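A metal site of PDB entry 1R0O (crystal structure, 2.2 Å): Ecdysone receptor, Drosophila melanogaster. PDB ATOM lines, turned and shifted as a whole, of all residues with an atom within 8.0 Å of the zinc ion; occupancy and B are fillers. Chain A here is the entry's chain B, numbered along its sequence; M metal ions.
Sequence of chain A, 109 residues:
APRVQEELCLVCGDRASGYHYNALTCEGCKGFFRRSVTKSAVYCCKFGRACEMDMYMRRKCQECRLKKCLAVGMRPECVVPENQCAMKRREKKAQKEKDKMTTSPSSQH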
ATOM      1  N   CYS A  44       6.133  11.146  15.289  1.00  0.00           N
ATOM      2  CA  CYS A  44       6.428  12.087  16.352  1.00  0.00           C
ATOM      3  C   CYS A  44       6.028  13.482  15.906  1.00  0.00           C
ATOM      4  O   CYS A  44       6.646  14.059  15.002  1.00  0.00           O
ATOM      5  CB  CYS A  44       7.929  12.046  16.673  1.00  0.00           C
ATOM      6  SG  CYS A  44       8.304  12.814  18.249  1.00  0.00           S
ATOM      7  N   CYS A  45       4.984  14.017  16.523  1.00  0.00           N
ATOM      8  CA  CYS A  45       4.500  15.352  16.201  1.00  0.00           C
ATOM      9  C   CYS A  45       5.567  16.400  16.479  1.00  0.00           C
ATOM     10  O   CYS A  45       6.021  16.545  17.623  1.00  0.00           O
ATOM     11  CB  CYS A  45       3.245  15.678  17.015  1.00  0.00           C
ATOM     12  SG  CYS A  45       2.743  17.415  16.965  1.00  0.00           S
ATOM     13  N   LYS A  46       5.976  17.131  15.454  1.00  0.00           N
ATOM     14  CA  LYS A  46       6.989  18.154  15.648  1.00  0.00           C
ATOM     15  C   LYS A  46       6.366  19.497  16.013  1.00  0.00           C
ATOM     16  O   LYS A  46       6.996  20.538  15.891  1.00  0.00           O
ATOM     17  CB  LYS A  46       7.825  18.297  14.385  1.00  0.00           C
ATOM     18  CG  LYS A  46       7.030  18.612  13.140  1.00  0.00           C
ATOM     19  CD  LYS A  46       7.770  18.116  11.908  1.00  0.00           C
ATOM     20  CE  LYS A  46       7.965  16.595  11.957  1.00  0.00           C
ATOM     21  NZ  LYS A  46       8.664  16.080  10.735  1.00  0.00           N
ATOM     22  N   PHE A  47       5.107  19.451  16.467  1.00  0.00           N
ATOM     23  CA  PHE A  47       4.405  20.656  16.885  1.00  0.00           C
ATOM     24  C   PHE A  47       3.994  20.465  18.340  1.00  0.00           C
ATOM     25  O   PHE A  47       4.757  19.923  19.137  1.00  0.00           O
ATOM     26  CB  PHE A  47       3.177  20.899  16.011  1.00  0.00           C
ATOM     27  CG  PHE A  47       3.500  21.067  14.556  1.00  0.00           C
ATOM     28  CD1 PHE A  47       3.141  20.085  13.632  1.00  0.00           C
ATOM     29  CD2 PHE A  47       4.169  22.209  14.105  1.00  0.00           C
ATOM     30  CE1 PHE A  47       3.460  20.231  12.279  1.00  0.00           C
ATOM     31  CE2 PHE A  47       4.487  22.369  12.761  1.00  0.00           C
ATOM     32  CZ  PHE A  47       4.134  21.380  11.839  1.00  0.00           C
ATOM     33  N   GLY A  48       2.781  20.864  18.682  1.00  0.00           N
ATOM     34  CA  GLY A  48       2.335  20.732  20.056  1.00  0.00           C
ATOM     35  C   GLY A  48       1.625  19.451  20.458  1.00  0.00           C
ATOM     36  O   GLY A  48       1.014  19.397  21.527  1.00  0.00           O
ATOM     37  N   ARG A  49       1.695  18.416  19.614  1.00  0.00           N
ATOM     38  CA  ARG A  49       1.049  17.132  19.927  1.00  0.00           C
ATOM     39  C   ARG A  49      -0.457  17.274  20.118  1.00  0.00           C
ATOM     40  O   ARG A  49      -1.080  16.459  20.796  1.00  0.00           O
ATOM     41  CB  ARG A  49       1.663  16.516  21.182  1.00  0.00           C
ATOM     42  CG  ARG A  49       2.828  15.566  20.903  1.00  0.00           C
ATOM     43  CD  ARG A  49       3.880  15.606  22.012  1.00  0.00           C
ATOM     44  NE  ARG A  49       3.341  15.445  23.365  1.00  0.00           N
ATOM     45  CZ  ARG A  49       2.721  14.357  23.808  1.00  0.00           C
ATOM     46  NH1 ARG A  49       2.532  13.307  23.006  1.00  0.00           N
ATOM     47  NH2 ARG A  49       2.285  14.304  25.061  1.00  0.00           N
ATOM     48  N   ALA A  50      -1.043  18.320  19.537  1.00  0.00           N
ATOM     49  CA  ALA A  50      -2.483  18.543  19.651  1.00  0.00           C
ATOM     50  C   ALA A  50      -3.049  19.115  18.366  1.00  0.00           C
ATOM     51  O   ALA A  50      -3.997  19.892  18.389  1.00  0.00           O
ATOM     52  CB  ALA A  50      -2.771  19.496  20.814  1.00  0.00           C
ATOM     53  N   CYS A  51      -2.457  18.725  17.232  1.00  0.00           N
ATOM     54  CA  CYS A  51      -2.896  19.204  15.937  1.00  0.00           C
ATOM     55  C   CYS A  51      -4.334  18.852  15.590  1.00  0.00           C
ATOM     56  O   CYS A  51      -4.765  17.713  15.769  1.00  0.00           O
ATOM     57  CB  CYS A  51      -1.987  18.654  14.837  1.00  0.00           C
ATOM     58  SG  CYS A  51      -0.257  19.076  15.015  1.00  0.00           S
ATOM     59  N   GLU A  52      -5.077  19.850  15.106  1.00  0.00           N
ATOM     60  CA  GLU A  52      -6.462  19.665  14.699  1.00  0.00           C
ATOM     61  C   GLU A  52      -6.396  19.310  13.206  1.00  0.00           C
ATOM     62  O   GLU A  52      -5.670  19.956  12.450  1.00  0.00           O
ATOM     63  CB  GLU A  52      -7.255  20.970  14.880  1.00  0.00           C
ATOM     64  CG  GLU A  52      -8.711  20.847  14.416  1.00  0.00           C
ATOM     65  CD  GLU A  52      -9.480  22.166  14.438  1.00  0.00           C
ATOM     66  OE1 GLU A  52      -9.737  22.706  15.547  1.00  0.00           O
ATOM     67  OE2 GLU A  52      -9.832  22.666  13.337  1.00  0.00           O
ATOM     68  N   MET A  53      -7.148  18.303  12.775  1.00  0.00           N
ATOM     69  CA  MET A  53      -7.118  17.870  11.386  1.00  0.00           C
ATOM     70  C   MET A  53      -8.065  18.560  10.392  1.00  0.00           C
ATOM     71  O   MET A  53      -9.213  18.891  10.718  1.00  0.00           O
ATOM     72  CB  MET A  53      -7.366  16.356  11.311  1.00  0.00           C
ATOM     73  CG  MET A  53      -6.291  15.500  11.934  1.00  0.00           C
ATOM     74  SD  MET A  53      -4.692  15.784  11.210  1.00  0.00           S
ATOM     75  CE  MET A  53      -4.846  14.752   9.892  1.00  0.00           C
ATOM     76  N   MET A  57      -3.782  20.266   7.366  1.00  0.00           N
ATOM     77  CA  MET A  57      -3.049  19.672   8.494  1.00  0.00           C
ATOM     78  C   MET A  57      -2.792  18.164   8.404  1.00  0.00           C
ATOM     79  O   MET A  57      -1.837  17.656   9.009  1.00  0.00           O
ATOM     80  CB  MET A  57      -3.821  19.964   9.781  1.00  0.00           C
ATOM     81  CG  MET A  57      -2.940  20.276  10.973  1.00  0.00           C
ATOM     82  SD  MET A  57      -1.815  21.659  10.628  1.00  0.00           S
ATOM     83  CE  MET A  57      -0.274  20.899  11.124  1.00  0.00           C
ATOM     84  N   LYS A  60       0.477  17.649   7.117  1.00  0.00           N
ATOM     85  CA  LYS A  60       1.504  18.232   7.973  1.00  0.00           C
ATOM     86  C   LYS A  60       1.873  17.460   9.243  1.00  0.00           C
ATOM     87  O   LYS A  60       2.971  17.645   9.756  1.00  0.00           O
ATOM     88  CB  LYS A  60       1.109  19.660   8.381  1.00  0.00           C
ATOM     89  CG  LYS A  60       1.126  20.699   7.242  1.00  0.00           C
ATOM     90  CD  LYS A  60       2.529  20.886   6.677  1.00  0.00           C
ATOM     91  CE  LYS A  60       2.607  22.103   5.758  1.00  0.00           C
ATOM     92  NZ  LYS A  60       3.937  22.232   5.083  1.00  0.00           N
ATOM     93  N   CYS A  61       0.988  16.613   9.756  1.00  0.00           N
ATOM     94  CA  CYS A  61       1.305  15.865  10.972  1.00  0.00           C
ATOM     95  C   CYS A  61       0.769  14.430  10.994  1.00  0.00           C
ATOM     96  O   CYS A  61      -0.373  14.173  11.363  1.00  0.00           O
ATOM     97  CB  CYS A  61       0.788  16.596  12.215  1.00  0.00           C
ATOM     98  SG  CYS A  61       1.409  15.884  13.759  1.00  0.00           S
ATOM     99  N   GLN A  62       1.639  13.498  10.614  1.00  0.00           N
ATOM    100  CA  GLN A  62       1.287  12.102  10.576  1.00  0.00           C
ATOM    101  C   GLN A  62       0.908  11.563  11.957  1.00  0.00           C
ATOM    102  O   GLN A  62      -0.040  10.781  12.076  1.00  0.00           O
ATOM    103  CB  GLN A  62       2.448  11.298   9.977  1.00  0.00           C
ATOM    104  CG  GLN A  62       3.097  11.969   8.751  1.00  0.00           C
ATOM    105  CD  GLN A  62       4.277  11.170   8.167  1.00  0.00           C
ATOM    106  OE1 GLN A  62       4.134  10.432   7.190  1.00  0.00           O
ATOM    107  NE2 GLN A  62       5.442  11.316   8.789  1.00  0.00           N
ATOM    108  N   GLU A  63       1.603  11.979  13.013  1.00  0.00           N
ATOM    109  CA  GLU A  63       1.247  11.446  14.328  1.00  0.00           C
ATOM    110  C   GLU A  63      -0.137  11.861  14.752  1.00  0.00           C
ATOM    111  O   GLU A  63      -0.906  11.022  15.210  1.00  0.00           O
ATOM    112  CB  GLU A  63       2.223  11.873  15.428  1.00  0.00           C
ATOM    113  CG  GLU A  63       1.867  11.213  16.774  1.00  0.00           C
ATOM    114  CD  GLU A  63       2.802  11.571  17.907  1.00  0.00           C
ATOM    115  OE1 GLU A  63       3.136  12.775  18.064  1.00  0.00           O
ATOM    116  OE2 GLU A  63       3.211  10.646  18.652  1.00  0.00           O
ATOM    117  N   CYS A  64      -0.458  13.149  14.622  1.00  0.00           N
ATOM    118  CA  CYS A  64      -1.785  13.597  15.029  1.00  0.00           C
ATOM    119  C   CYS A  64      -2.863  13.046  14.089  1.00  0.00           C
ATOM    120  O   CYS A  64      -3.996  12.810  14.512  1.00  0.00           O
ATOM    121  CB  CYS A  64      -1.834  15.128  15.137  1.00  0.00           C
ATOM    122  SG  CYS A  64      -0.966  15.762  16.654  1.00  0.00           S
ATOM    123  N   ARG A  65      -2.509  12.813  12.827  1.00  0.00           N
ATOM    124  CA  ARG A  65      -3.473  12.264  11.863  1.00  0.00           C
ATOM    125  C   ARG A  65      -3.752  10.796  12.212  1.00  0.00           C
ATOM    126  O   ARG A  65      -4.908  10.367  12.188  1.00  0.00           O
ATOM    127  CB  ARG A  65      -2.931  12.334  10.439  1.00  0.00           C
ATOM    128  CG  ARG A  65      -3.900  11.842   9.391  1.00  0.00           C
ATOM    129  CD  ARG A  65      -3.260  11.898   8.011  1.00  0.00           C
ATOM    130  NE  ARG A  65      -4.242  11.712   6.939  1.00  0.00           N
ATOM    131  CZ  ARG A  65      -3.964  11.781   5.648  1.00  0.00           C
ATOM    132  NH1 ARG A  65      -2.726  12.019   5.239  1.00  0.00           N
ATOM    133  NH2 ARG A  65      -4.930  11.635   4.764  1.00  0.00           N
ATOM    134  N   LYS A  67      -3.506   9.374  15.138  1.00  0.00           N
ATOM    135  CA  LYS A  67      -4.272   9.341  16.376  1.00  0.00           C
ATOM    136  C   LYS A  67      -5.750   9.613  16.111  1.00  0.00           C
ATOM    137  O   LYS A  67      -6.648   8.930  16.632  1.00  0.00           O
ATOM    138  CB  LYS A  67      -3.744  10.376  17.371  1.00  0.00           C
ATOM    139  CG  LYS A  67      -2.418  10.037  18.021  1.00  0.00           C
ATOM    140  CD  LYS A  67      -2.046  11.159  18.989  1.00  0.00           C
ATOM    141  CE  LYS A  67      -0.655  11.008  19.562  1.00  0.00           C
ATOM    142  NZ  LYS A  67      -0.308  12.169  20.432  1.00  0.00           N
HETATM  143 ZN    ZN M   1       0.685  16.997  15.580  1.00  0.00          ZN
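Four residues have an atom within 4 Å of the zinc ion: Cys 45, Cys 51, Cys 61 and Cys 64.
Along chain A the residues within 4 Å of the zinc ion span positions 45 to 64.
The nearest printed residue that does not touch the zinc ion is Arg 49 (4.4 Å).
The zinc ion is bound by the side-chain sulfur of Cys 61 (2.3 Å), the side-chain sulfur of Cys 64 (2.3 Å), the side-chain sulfur of Cys 51 (2.4 Å) and the side-chain sulfur of Cys 45 (2.5 Å).
The zinc ion has four donor atoms within binding distance.
SG of Cys 45 lies close to N of Arg 49 (3.0 Å).
N of Phe 47 lies close to SG of Cys 45 (3.2 Å).
N of Cys 45 sits at hydrogen-bond distance from OE1 of Glu 63 (2.7 Å).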
